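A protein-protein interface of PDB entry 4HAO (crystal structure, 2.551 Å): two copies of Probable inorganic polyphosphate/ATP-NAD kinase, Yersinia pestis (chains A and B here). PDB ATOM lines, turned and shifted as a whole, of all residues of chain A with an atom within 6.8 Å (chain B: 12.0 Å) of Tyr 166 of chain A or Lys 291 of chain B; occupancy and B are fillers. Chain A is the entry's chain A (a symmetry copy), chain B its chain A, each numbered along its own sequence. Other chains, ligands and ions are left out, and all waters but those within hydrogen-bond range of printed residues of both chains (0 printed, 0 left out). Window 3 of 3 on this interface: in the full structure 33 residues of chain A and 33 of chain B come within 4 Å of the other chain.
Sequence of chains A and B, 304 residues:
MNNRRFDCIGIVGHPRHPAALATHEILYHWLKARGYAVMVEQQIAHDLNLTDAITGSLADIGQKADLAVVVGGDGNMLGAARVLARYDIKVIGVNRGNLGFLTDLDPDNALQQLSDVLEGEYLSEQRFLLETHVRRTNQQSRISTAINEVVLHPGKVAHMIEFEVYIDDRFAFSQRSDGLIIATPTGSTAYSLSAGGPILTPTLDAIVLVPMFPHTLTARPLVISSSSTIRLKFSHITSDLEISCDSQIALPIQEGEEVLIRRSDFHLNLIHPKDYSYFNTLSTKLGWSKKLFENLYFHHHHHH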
ATOM      1  N   GLU A 164     -20.549  -9.722  29.362  1.00  0.00           N
ATOM      2  CA  GLU A 164     -21.125  -8.395  29.321  1.00  0.00           C
ATOM      3  C   GLU A 164     -19.988  -7.405  29.350  1.00  0.00           C
ATOM      4  O   GLU A 164     -18.927  -7.669  29.949  1.00  0.00           O
ATOM      5  CB  GLU A 164     -22.050  -8.172  30.507  1.00  0.00           C
ATOM      6  CG  GLU A 164     -23.224  -9.097  30.524  1.00  0.00           C
ATOM      7  CD  GLU A 164     -24.005  -8.960  31.785  1.00  0.00           C
ATOM      8  OE1 GLU A 164     -23.536  -8.233  32.690  1.00  0.00           O
ATOM      9  OE2 GLU A 164     -25.088  -9.576  31.875  1.00  0.00           O
ATOM     10  N   VAL A 165     -20.212  -6.275  28.688  1.00  0.00           N
ATOM     11  CA  VAL A 165     -19.197  -5.262  28.515  1.00  0.00           C
ATOM     12  C   VAL A 165     -19.652  -3.989  29.196  1.00  0.00           C
ATOM     13  O   VAL A 165     -20.679  -3.433  28.836  1.00  0.00           O
ATOM     14  CB  VAL A 165     -18.988  -4.985  27.043  1.00  0.00           C
ATOM     15  CG1 VAL A 165     -18.102  -3.757  26.847  1.00  0.00           C
ATOM     16  CG2 VAL A 165     -18.419  -6.211  26.355  1.00  0.00           C
ATOM     17  N   TYR A 166     -18.903  -3.532  30.190  1.00  0.00           N
ATOM     18  CA  TYR A 166     -19.236  -2.288  30.881  1.00  0.00           C
ATOM     19  C   TYR A 166     -18.270  -1.205  30.445  1.00  0.00           C
ATOM     20  O   TYR A 166     -17.049  -1.407  30.472  1.00  0.00           O
ATOM     21  CB  TYR A 166     -19.178  -2.454  32.402  1.00  0.00           C
ATOM     22  CG  TYR A 166     -20.312  -3.268  32.972  1.00  0.00           C
ATOM     23  CD1 TYR A 166     -21.233  -2.694  33.827  1.00  0.00           C
ATOM     24  CD2 TYR A 166     -20.472  -4.612  32.640  1.00  0.00           C
ATOM     25  CE1 TYR A 166     -22.278  -3.431  34.344  1.00  0.00           C
ATOM     26  CE2 TYR A 166     -21.518  -5.358  33.145  1.00  0.00           C
ATOM     27  CZ  TYR A 166     -22.415  -4.763  33.997  1.00  0.00           C
ATOM     28  OH  TYR A 166     -23.459  -5.497  34.510  1.00  0.00           O
ATOM     29  N   ILE A 167     -18.814  -0.062  30.022  1.00  0.00           N
ATOM     30  CA  ILE A 167     -17.971   1.078  29.678  1.00  0.00           C
ATOM     31  C   ILE A 167     -18.168   2.211  30.671  1.00  0.00           C
ATOM     32  O   ILE A 167     -19.276   2.691  30.861  1.00  0.00           O
ATOM     33  CB  ILE A 167     -18.182   1.550  28.234  1.00  0.00           C
ATOM     34  CG1 ILE A 167     -17.896   0.397  27.268  1.00  0.00           C
ATOM     35  CG2 ILE A 167     -17.272   2.724  27.928  1.00  0.00           C
ATOM     36  CD1 ILE A 167     -17.868   0.784  25.821  1.00  0.00           C
ATOM     37  N   ASP A 168     -17.078   2.605  31.323  1.00  0.00           N
ATOM     38  CA  ASP A 168     -17.103   3.638  32.358  1.00  0.00           C
ATOM     39  C   ASP A 168     -18.111   3.317  33.465  1.00  0.00           C
ATOM     40  O   ASP A 168     -18.946   4.151  33.815  1.00  0.00           O
ATOM     41  CB  ASP A 168     -17.344   5.025  31.745  1.00  0.00           C
ATOM     42  CG  ASP A 168     -16.333   5.357  30.662  1.00  0.00           C
ATOM     43  OD1 ASP A 168     -15.617   4.439  30.235  1.00  0.00           O
ATOM     44  OD2 ASP A 168     -16.239   6.510  30.221  1.00  0.00           O
ATOM     45  N   ASP A 169     -18.017   2.093  33.988  1.00  0.00           N
ATOM     46  CA  ASP A 169     -18.829   1.610  35.110  1.00  0.00           C
ATOM     47  C   ASP A 169     -20.299   1.360  34.790  1.00  0.00           C
ATOM     48  O   ASP A 169     -21.072   0.994  35.671  1.00  0.00           O
ATOM     49  CB  ASP A 169     -18.720   2.546  36.314  1.00  0.00           C
ATOM     50  CG  ASP A 169     -17.400   2.411  37.038  1.00  0.00           C
ATOM     51  OD1 ASP A 169     -16.855   1.284  37.077  1.00  0.00           O
ATOM     52  OD2 ASP A 169     -16.911   3.433  37.573  1.00  0.00           O
ATOM     53  N   ARG A 170     -20.696   1.560  33.542  1.00  0.00           N
ATOM     54  CA  ARG A 170     -22.097   1.389  33.201  1.00  0.00           C
ATOM     55  C   ARG A 170     -22.261   0.315  32.142  1.00  0.00           C
ATOM     56  O   ARG A 170     -21.415   0.173  31.261  1.00  0.00           O
ATOM     57  CB  ARG A 170     -22.720   2.734  32.807  1.00  0.00           C
ATOM     58  CG  ARG A 170     -22.810   3.672  34.018  1.00  0.00           C
ATOM     59  CD  ARG A 170     -23.142   5.127  33.696  1.00  0.00           C
ATOM     60  NE  ARG A 170     -23.258   5.916  34.931  1.00  0.00           N
ATOM     61  CZ  ARG A 170     -23.603   7.204  34.987  1.00  0.00           C
ATOM     62  NH1 ARG A 170     -23.870   7.876  33.874  1.00  0.00           N
ATOM     63  NH2 ARG A 170     -23.682   7.823  36.160  1.00  0.00           N
ATOM     64  N   PHE A 171     -23.326  -0.471  32.262  1.00  0.00           N
ATOM     65  CA  PHE A 171     -23.553  -1.590  31.357  1.00  0.00           C
ATOM     66  C   PHE A 171     -23.783  -1.124  29.917  1.00  0.00           C
ATOM     67  O   PHE A 171     -24.742  -0.426  29.635  1.00  0.00           O
ATOM     68  CB  PHE A 171     -24.736  -2.446  31.819  1.00  0.00           C
ATOM     69  CG  PHE A 171     -25.197  -3.443  30.787  1.00  0.00           C
ATOM     70  CD1 PHE A 171     -24.430  -4.564  30.490  1.00  0.00           C
ATOM     71  CD2 PHE A 171     -26.383  -3.255  30.099  1.00  0.00           C
ATOM     72  CE1 PHE A 171     -24.840  -5.479  29.534  1.00  0.00           C
ATOM     73  CE2 PHE A 171     -26.796  -4.168  29.135  1.00  0.00           C
ATOM     74  CZ  PHE A 171     -26.022  -5.283  28.858  1.00  0.00           C
ATOM     75  N   ALA A 172     -22.898  -1.524  29.013  1.00  0.00           N
ATOM     76  CA  ALA A 172     -23.028  -1.184  27.610  1.00  0.00           C
ATOM     77  C   ALA A 172     -23.844  -2.220  26.829  1.00  0.00           C
ATOM     78  O   ALA A 172     -24.944  -1.918  26.367  1.00  0.00           O
ATOM     79  CB  ALA A 172     -21.671  -0.993  26.986  1.00  0.00           C
ATOM     80  N   PHE A 173     -23.323  -3.431  26.679  1.00  0.00           N
ATOM     81  CA  PHE A 173     -24.019  -4.447  25.895  1.00  0.00           C
ATOM     82  C   PHE A 173     -23.559  -5.858  26.278  1.00  0.00           C
ATOM     83  O   PHE A 173     -22.462  -6.037  26.801  1.00  0.00           O
ATOM     84  CB  PHE A 173     -23.775  -4.214  24.400  1.00  0.00           C
ATOM     85  CG  PHE A 173     -22.309  -4.136  24.029  1.00  0.00           C
ATOM     86  CD1 PHE A 173     -21.626  -5.263  23.605  1.00  0.00           C
ATOM     87  CD2 PHE A 173     -21.615  -2.940  24.129  1.00  0.00           C
ATOM     88  CE1 PHE A 173     -20.282  -5.195  23.275  1.00  0.00           C
ATOM     89  CE2 PHE A 173     -20.278  -2.864  23.809  1.00  0.00           C
ATOM     90  CZ  PHE A 173     -19.610  -3.985  23.379  1.00  0.00           C
ATOM     91  N   SER A 174     -24.402  -6.853  26.013  1.00  0.00           N
ATOM     92  CA  SER A 174     -24.010  -8.251  26.148  1.00  0.00           C
ATOM     93  C   SER A 174     -23.401  -8.730  24.849  1.00  0.00           C
ATOM     94  O   SER A 174     -23.429  -8.014  23.847  1.00  0.00           O
ATOM     95  CB  SER A 174     -25.214  -9.126  26.462  1.00  0.00           C
ATOM     96  OG  SER A 174     -25.605  -9.009  27.814  1.00  0.00           O
ATOM     97  N   THR A 229     -12.979   3.486  30.387  1.00  0.00           N
ATOM     98  CA  THR A 229     -12.695   2.241  31.081  1.00  0.00           C
ATOM     99  C   THR A 229     -13.591   1.121  30.533  1.00  0.00           C
ATOM    100  O   THR A 229     -14.740   1.380  30.178  1.00  0.00           O
ATOM    101  CB  THR A 229     -13.013   2.437  32.565  1.00  0.00           C
ATOM    102  OG1 THR A 229     -11.798   2.646  33.297  1.00  0.00           O
ATOM    103  CG2 THR A 229     -13.787   1.254  33.134  1.00  0.00           C
ATOM    104  N   ILE A 230     -13.072  -0.108  30.457  1.00  0.00           N
ATOM    105  CA  ILE A 230     -13.839  -1.268  29.996  1.00  0.00           C
ATOM    106  C   ILE A 230     -13.829  -2.408  31.027  1.00  0.00           C
ATOM    107  O   ILE A 230     -12.792  -2.727  31.610  1.00  0.00           O
ATOM    108  CB  ILE A 230     -13.275  -1.816  28.676  1.00  0.00           C
ATOM    109  CG1 ILE A 230     -13.066  -0.693  27.659  1.00  0.00           C
ATOM    110  CG2 ILE A 230     -14.202  -2.885  28.077  1.00  0.00           C
ATOM    111  CD1 ILE A 230     -12.573  -1.190  26.313  1.00  0.00           C
ATOM    112  N   ARG A 231     -14.988  -3.020  31.258  1.00  0.00           N
ATOM    113  CA  ARG A 231     -15.100  -4.129  32.202  1.00  0.00           C
ATOM    114  C   ARG A 231     -15.776  -5.338  31.582  1.00  0.00           C
ATOM    115  O   ARG A 231     -16.857  -5.233  31.015  1.00  0.00           O
ATOM    116  CB  ARG A 231     -15.844  -3.721  33.481  1.00  0.00           C
ATOM    117  CG  ARG A 231     -14.989  -2.907  34.442  1.00  0.00           C
ATOM    118  CD  ARG A 231     -15.451  -3.027  35.886  1.00  0.00           C
ATOM    119  NE  ARG A 231     -16.450  -2.033  36.262  1.00  0.00           N
ATOM    120  CZ  ARG A 231     -17.602  -2.337  36.856  1.00  0.00           C
ATOM    121  NH1 ARG A 231     -17.890  -3.607  37.125  1.00  0.00           N
ATOM    122  NH2 ARG A 231     -18.467  -1.380  37.185  1.00  0.00           N
ATOM    123  N   LEU A 232     -15.132  -6.493  31.710  1.00  0.00           N
ATOM    124  CA  LEU A 232     -15.686  -7.726  31.192  1.00  0.00           C
ATOM    125  C   LEU A 232     -16.228  -8.552  32.343  1.00  0.00           C
ATOM    126  O   LEU A 232     -15.510  -8.853  33.285  1.00  0.00           O
ATOM    127  CB  LEU A 232     -14.624  -8.475  30.386  1.00  0.00           C
ATOM    128  CG  LEU A 232     -13.969  -7.627  29.284  1.00  0.00           C
ATOM    129  CD1 LEU A 232     -12.999  -8.447  28.453  1.00  0.00           C
ATOM    130  CD2 LEU A 232     -15.000  -6.980  28.380  1.00  0.00           C
ATOM    131  N   LYS A 233     -17.511  -8.884  32.289  1.00  0.00           N
ATOM    132  CA  LYS A 233     -18.112  -9.731  33.310  1.00  0.00           C
ATOM    133  C   LYS A 233     -18.602 -11.006  32.660  1.00  0.00           C
ATOM    134  O   LYS A 233     -19.096 -10.979  31.527  1.00  0.00           O
ATOM    135  CB  LYS A 233     -19.272  -9.035  34.031  1.00  0.00           C
ATOM    136  CG  LYS A 233     -18.879  -7.922  34.971  1.00  0.00           C
ATOM    137  CD  LYS A 233     -20.094  -7.427  35.750  1.00  0.00           C
ATOM    138  CE  LYS A 233     -19.745  -6.272  36.691  1.00  0.00           C
ATOM    139  NZ  LYS A 233     -20.932  -5.735  37.421  1.00  0.00           N
ATOM    140  N   GLU A 258     -13.265 -10.689  37.008  1.00  0.00           N
ATOM    141  CA  GLU A 258     -13.595  -9.772  35.940  1.00  0.00           C
ATOM    142  C   GLU A 258     -12.310  -9.235  35.333  1.00  0.00           C
ATOM    143  O   GLU A 258     -11.264  -9.250  35.980  1.00  0.00           O
ATOM    144  CB  GLU A 258     -14.448  -8.637  36.479  1.00  0.00           C
ATOM    145  CG  GLU A 258     -15.698  -9.114  37.177  1.00  0.00           C
ATOM    146  CD  GLU A 258     -16.630  -7.975  37.536  1.00  0.00           C
ATOM    147  OE1 GLU A 258     -16.370  -6.836  37.092  1.00  0.00           O
ATOM    148  OE2 GLU A 258     -17.621  -8.221  38.253  1.00  0.00           O
ATOM    149  N   THR B 201     -18.528   6.439  19.143  1.00  0.00           N
ATOM    150  CA  THR B 201     -19.216   6.930  20.322  1.00  0.00           C
ATOM    151  C   THR B 201     -19.445   8.446  20.138  1.00  0.00           C
ATOM    152  O   THR B 201     -18.575   9.146  19.627  1.00  0.00           O
ATOM    153  CB  THR B 201     -18.387   6.550  21.573  1.00  0.00           C
ATOM    154  OG1 THR B 201     -19.220   6.523  22.734  1.00  0.00           O
ATOM    155  CG2 THR B 201     -17.214   7.483  21.778  1.00  0.00           C
ATOM    156  N   SER B 277     -29.086   6.737  28.294  1.00  0.00           N
ATOM    157  CA  SER B 277     -27.707   6.347  28.045  1.00  0.00           C
ATOM    158  C   SER B 277     -27.525   5.967  26.578  1.00  0.00           C
ATOM    159  O   SER B 277     -28.390   5.338  25.974  1.00  0.00           O
ATOM    160  CB  SER B 277     -27.284   5.191  28.945  1.00  0.00           C
ATOM    161  OG  SER B 277     -27.374   3.959  28.251  1.00  0.00           O
ATOM    162  N   TYR B 278     -26.388   6.346  26.012  1.00  0.00           N
ATOM    163  CA  TYR B 278     -26.117   6.072  24.611  1.00  0.00           C
ATOM    164  C   TYR B 278     -26.243   4.586  24.277  1.00  0.00           C
ATOM    165  O   TYR B 278     -26.997   4.217  23.361  1.00  0.00           O
ATOM    166  CB  TYR B 278     -24.740   6.603  24.211  1.00  0.00           C
ATOM    167  CG  TYR B 278     -24.295   6.142  22.843  1.00  0.00           C
ATOM    168  CD1 TYR B 278     -24.974   6.549  21.705  1.00  0.00           C
ATOM    169  CD2 TYR B 278     -23.198   5.282  22.691  1.00  0.00           C
ATOM    170  CE1 TYR B 278     -24.583   6.138  20.456  1.00  0.00           C
ATOM    171  CE2 TYR B 278     -22.797   4.862  21.436  1.00  0.00           C
ATOM    172  CZ  TYR B 278     -23.498   5.292  20.321  1.00  0.00           C
ATOM    173  OH  TYR B 278     -23.118   4.888  19.055  1.00  0.00           O
ATOM    174  N   PHE B 279     -25.523   3.741  25.027  1.00  0.00           N
ATOM    175  CA  PHE B 279     -25.443   2.306  24.727  1.00  0.00           C
ATOM    176  C   PHE B 279     -26.787   1.588  24.755  1.00  0.00           C
ATOM    177  O   PHE B 279     -27.018   0.664  23.983  1.00  0.00           O
ATOM    178  CB  PHE B 279     -24.394   1.609  25.595  1.00  0.00           C
ATOM    179  CG  PHE B 279     -22.986   2.020  25.261  1.00  0.00           C
ATOM    180  CD1 PHE B 279     -22.450   1.724  24.011  1.00  0.00           C
ATOM    181  CD2 PHE B 279     -22.212   2.729  26.176  1.00  0.00           C
ATOM    182  CE1 PHE B 279     -21.180   2.121  23.671  1.00  0.00           C
ATOM    183  CE2 PHE B 279     -20.922   3.123  25.851  1.00  0.00           C
ATOM    184  CZ  PHE B 279     -20.408   2.821  24.583  1.00  0.00           C
ATOM    185  N   ASN B 280     -27.687   2.042  25.616  1.00  0.00           N
ATOM    186  CA  ASN B 280     -29.070   1.560  25.607  1.00  0.00           C
ATOM    187  C   ASN B 280     -29.859   1.985  24.347  1.00  0.00           C
ATOM    188  O   ASN B 280     -30.635   1.197  23.787  1.00  0.00           O
ATOM    189  CB  ASN B 280     -29.792   2.015  26.882  1.00  0.00           C
ATOM    190  CG  ASN B 280     -31.210   1.508  26.955  1.00  0.00           C
ATOM    191  OD1 ASN B 280     -31.447   0.335  27.261  1.00  0.00           O
ATOM    192  ND2 ASN B 280     -32.171   2.387  26.667  1.00  0.00           N
ATOM    193  N   THR B 281     -29.666   3.229  23.912  1.00  0.00           N
ATOM    194  CA  THR B 281     -30.235   3.694  22.648  1.00  0.00           C
ATOM    195  C   THR B 281     -29.691   2.850  21.499  1.00  0.00           C
ATOM    196  O   THR B 281     -30.443   2.312  20.692  1.00  0.00           O
ATOM    197  CB  THR B 281     -29.879   5.172  22.396  1.00  0.00           C
ATOM    198  OG1 THR B 281     -30.447   5.981  23.434  1.00  0.00           O
ATOM    199  CG2 THR B 281     -30.408   5.642  21.028  1.00  0.00           C
ATOM    200  N   LEU B 282     -28.369   2.733  21.456  1.00  0.00           N
ATOM    201  CA  LEU B 282     -27.659   1.953  20.443  1.00  0.00           C
ATOM    202  C   LEU B 282     -28.113   0.502  20.356  1.00  0.00           C
ATOM    203  O   LEU B 282     -28.340  -0.020  19.277  1.00  0.00           O
ATOM    204  CB  LEU B 282     -26.155   1.975  20.731  1.00  0.00           C
ATOM    205  CG  LEU B 282     -25.288   1.479  19.575  1.00  0.00           C
ATOM    206  CD1 LEU B 282     -25.321   2.503  18.440  1.00  0.00           C
ATOM    207  CD2 LEU B 282     -23.847   1.183  20.015  1.00  0.00           C
ATOM    208  N   SER B 283     -28.225  -0.161  21.494  1.00  0.00           N
ATOM    209  CA  SER B 283     -28.575  -1.570  21.490  1.00  0.00           C
ATOM    210  C   SER B 283     -30.001  -1.789  20.996  1.00  0.00           C
ATOM    211  O   SER B 283     -30.238  -2.648  20.149  1.00  0.00           O
ATOM    212  CB  SER B 283     -28.347  -2.200  22.873  1.00  0.00           C
ATOM    213  OG  SER B 283     -28.775  -1.329  23.904  1.00  0.00           O
ATOM    214  N   THR B 284     -30.945  -1.006  21.509  1.00  0.00           N
ATOM    215  CA  THR B 284     -32.328  -1.111  21.068  1.00  0.00           C
ATOM    216  C   THR B 284     -32.441  -0.817  19.573  1.00  0.00           C
ATOM    217  O   THR B 284     -33.224  -1.442  18.865  1.00  0.00           O
ATOM    218  CB  THR B 284     -33.240  -0.146  21.847  1.00  0.00           C
ATOM    219  OG1 THR B 284     -32.589   1.126  21.968  1.00  0.00           O
ATOM    220  CG2 THR B 284     -33.507  -0.674  23.234  1.00  0.00           C
ATOM    221  N   GLY B 287     -30.320  -3.825  17.758  1.00  0.00           N
ATOM    222  CA  GLY B 287     -30.715  -5.180  18.103  1.00  0.00           C
ATOM    223  C   GLY B 287     -29.626  -5.946  18.839  1.00  0.00           C
ATOM    224  O   GLY B 287     -29.399  -7.126  18.589  1.00  0.00           O
ATOM    225  N   TRP B 288     -28.942  -5.268  19.753  1.00  0.00           N
ATOM    226  CA  TRP B 288     -27.894  -5.888  20.532  1.00  0.00           C
ATOM    227  C   TRP B 288     -28.480  -6.513  21.783  1.00  0.00           C
ATOM    228  O   TRP B 288     -29.553  -6.103  22.237  1.00  0.00           O
ATOM    229  CB  TRP B 288     -26.850  -4.851  20.903  1.00  0.00           C
ATOM    230  CG  TRP B 288     -26.019  -4.479  19.745  1.00  0.00           C
ATOM    231  CD1 TRP B 288     -26.190  -4.882  18.457  1.00  0.00           C
ATOM    232  CD2 TRP B 288     -24.872  -3.632  19.753  1.00  0.00           C
ATOM    233  NE1 TRP B 288     -25.216  -4.345  17.660  1.00  0.00           N
ATOM    234  CE2 TRP B 288     -24.396  -3.568  18.429  1.00  0.00           C
ATOM    235  CE3 TRP B 288     -24.200  -2.919  20.750  1.00  0.00           C
ATOM    236  CZ2 TRP B 288     -23.277  -2.824  18.077  1.00  0.00           C
ATOM    237  CZ3 TRP B 288     -23.085  -2.184  20.400  1.00  0.00           C
ATOM    238  CH2 TRP B 288     -22.633  -2.143  19.074  1.00  0.00           C
ATOM    239  N   SER B 289     -27.775  -7.505  22.332  1.00  0.00           N
ATOM    240  CA  SER B 289     -28.208  -8.176  23.551  1.00  0.00           C
ATOM    241  C   SER B 289     -28.171  -7.267  24.761  1.00  0.00           C
ATOM    242  O   SER B 289     -27.230  -6.483  24.955  1.00  0.00           O
ATOM    243  CB  SER B 289     -27.346  -9.397  23.831  1.00  0.00           C
ATOM    244  OG  SER B 289     -27.780 -10.486  23.057  1.00  0.00           O
ATOM    245  N   LYS B 290     -29.212  -7.385  25.575  1.00  0.00           N
ATOM    246  CA  LYS B 290     -29.283  -6.664  26.828  1.00  0.00           C
ATOM    247  C   LYS B 290     -28.609  -7.514  27.873  1.00  0.00           C
ATOM    248  O   LYS B 290     -28.027  -8.545  27.546  1.00  0.00           O
ATOM    249  CB  LYS B 290     -30.735  -6.388  27.208  1.00  0.00           C
ATOM    250  CG  LYS B 290     -31.402  -5.316  26.338  1.00  0.00           C
ATOM    251  CD  LYS B 290     -30.621  -3.996  26.386  1.00  0.00           C
ATOM    252  CE  LYS B 290     -31.164  -2.963  25.395  1.00  0.00           C
ATOM    253  NZ  LYS B 290     -32.539  -2.492  25.717  1.00  0.00           N
ATOM    254  N   LYS B 291     -28.694  -7.082  29.123  1.00  0.00           N
ATOM    255  CA  LYS B 291     -28.044  -7.775  30.228  1.00  0.00           C
ATOM    256  C   LYS B 291     -28.348  -9.278  30.224  1.00  0.00           C
ATOM    257  O   LYS B 291     -29.506  -9.685  30.137  1.00  0.00           O
ATOM    258  CB  LYS B 291     -28.451  -7.131  31.556  1.00  0.00           C
ATOM    259  CG  LYS B 291     -27.550  -7.484  32.720  1.00  0.00           C
ATOM    260  CD  LYS B 291     -27.711  -6.484  33.852  1.00  0.00           C
ATOM    261  CE  LYS B 291     -27.072  -5.141  33.520  1.00  0.00           C
ATOM    262  NZ  LYS B 291     -26.486  -4.491  34.744  1.00  0.00           N
ATOM    263  N   LEU B 292     -27.297 -10.094  30.288  1.00  0.00           N
ATOM    264  CA  LEU B 292     -27.456 -11.548  30.249  1.00  0.00           C
ATOM    265  C   LEU B 292     -27.552 -12.228  31.620  1.00  0.00           C
ATOM    266  O   LEU B 292     -28.141 -13.301  31.729  1.00  0.00           O
ATOM    267  CB  LEU B 292     -26.353 -12.212  29.418  1.00  0.00           C
ATOM    268  CG  LEU B 292     -26.448 -12.094  27.894  1.00  0.00           C
ATOM    269  CD1 LEU B 292     -25.871 -13.337  27.218  1.00  0.00           C
ATOM    270  CD2 LEU B 292     -27.881 -11.802  27.425  1.00  0.00           C
ATOM    271  N   PHE B 293     -26.966 -11.632  32.654  1.00  0.00           N
ATOM    272  CA  PHE B 293     -27.070 -12.206  33.996  1.00  0.00           C
ATOM    273  C   PHE B 293     -27.406 -11.150  35.038  1.00  0.00           C
ATOM    274  O   PHE B 293     -27.340  -9.955  34.761  1.00  0.00           O
ATOM    275  CB  PHE B 293     -25.801 -12.973  34.407  1.00  0.00           C
ATOM    276  CG  PHE B 293     -24.697 -12.953  33.379  1.00  0.00           C
ATOM    277  CD1 PHE B 293     -24.747 -13.780  32.264  1.00  0.00           C
ATOM    278  CD2 PHE B 293     -23.593 -12.129  33.542  1.00  0.00           C
ATOM    279  CE1 PHE B 293     -23.730 -13.760  31.313  1.00  0.00           C
ATOM    280  CE2 PHE B 293     -22.572 -12.110  32.601  1.00  0.00           C
ATOM    281  CZ  PHE B 293     -22.639 -12.930  31.488  1.00  0.00           C
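N of Ser 174 of chain A sits at hydrogen-bond distance from O of Ser 289 of chain B (3.0 Å). OG of Ser 174 of chain A is in hydrogen-bond range of O of Lys 290 of chain B (2.5 Å). The side-chain amino group (NZ) of Lys 291 of chain B is in hydrogen-bond range of the side-chain hydroxyl (OH) of Tyr 166 of chain A, at 3.2 Å. N of Leu 292 of chain B is in hydrogen-bond range of OE2 of Glu 164 of chain A (2.8 Å). N of Leu 292 of chain B is in hydrogen-bond range of OG of Ser 174 of chain A (3.2 Å). The side-chain carboxylate (OE2) of Glu 164 of chain A sits at hydrogen-bond distance from the backbone NH (N) of Phe 293 of chain B.
The backbone carbonyl oxygen (O) of Ser 283 of chain B sits at hydrogen-bond distance from the backbone NH (N) of Trp 288 of chain B (2.9 Å). The side-chain carboxylate (OE1) of Glu 164 of chain A is in hydrogen-bond range of the side-chain hydroxyl (OH) of Tyr 166 of chain A (3.3 Å). The backbone NH of Glu 164 of chain A lies within hydrogen-bond range of the backbone carbonyl oxygen of Lys 233 of chain A (2.9 Å). The backbone carbonyl oxygen (O) of Val 165 of chain A is in hydrogen-bond range of the backbone NH (N) of Ala 172 of chain A (2.9 Å). N of Val 165 of chain A sits at hydrogen-bond distance from O of Phe 173 of chain A, 2.9 Å away. O of Tyr 166 of chain A lies within hydrogen-bond range of N of Arg 231 of chain A, 2.7 Å away.
Lys 291 of chain B touches Glu 164 of chain A (CG to OE2, 3.3 Å). Phe 279 of chain B touches Ile 167 of chain A (CZ to CD1, 3.5 Å). Lys 290 of chain B touches Phe 171 of chain A. Phe 171 of chain A touches Lys 291 of chain B. Ala 172 of chain A touches Phe 279 of chain B (O to CB, 3.7 Å). Phe 173 of chain A touches Trp 288 of chain B. Phe 173 of chain A touches Ser 289 of chain B (CA to O, 3.9 Å). Ser 174 of chain A touches Lys 291 of chain B. O of Lys 233 of chain A touches CE2 of Phe 293 of chain B, 3.8 Å away.
Of chain B, only Lys 291 (3.3 Å), Leu 292 (2.8 Å) and Phe 293 (2.9 Å) come within 4 Å of Glu 164 of chain A. No residue of chain B comes within 4 Å of Val 165 of chain A. Of chain B, only Trp 288 and Ser 289 come within 4 Å of Phe 173 of chain A. Of the printed residues of chain B, Ser 174 of chain A touches Ser 289, Lys 290, Lys 291 and Leu 292. No residue of chain B comes within 4 Å of Thr 229 of chain A. No residue of chain B comes within 4 Å of Ile 230 of chain A. Of chain B, only Phe 293 comes within 4 Å of Lys 233 of chain A. Of the printed residues of chain A, Phe 279 of chain B touches Ile 167 and Ala 172. Of the printed residues of chain A, Ser 289 of chain B touches Phe 173 and Ser 174. Of the printed residues of chain A, Lys 290 of chain B touches Phe 171 and Ser 174. Of chain A, only Glu 164, Tyr 166, Phe 171 and Ser 174 come within 4 Å of Lys 291 of chain B. Of the printed residues of chain A, Phe 293 of chain B touches Glu 164 (2.9 Å) and Lys 233 (3.8 Å). The nearest residue of chain B that does not touch Tyr 166 of chain A is Phe 293 of chain B (5.9 Å). The nearest printed residue of chain A that does not touch Lys 290 of chain B is Glu 164 of chain A (5.3 Å).
Of the 16 printed residues of chain B, 7 touch a printed residue of chain A. Hydrophobic or aromatic side chains of chain B within 4 Å of the printed part of chain A: Phe 279, Trp 288, Leu 292 and Phe 293. Hydrophobic or aromatic side chains of chain A that line the printed part of chain B: Tyr 166, Ile 167, Phe 171, Ala 172 and Phe 173. Among the printed residues, 15 pairs touch across the chains. Among the printed residues, no Asp or Glu carboxylate lies within 4 Å of a Lys or Arg side-chain nitrogen of the other chain.
No position is printed for both chains.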
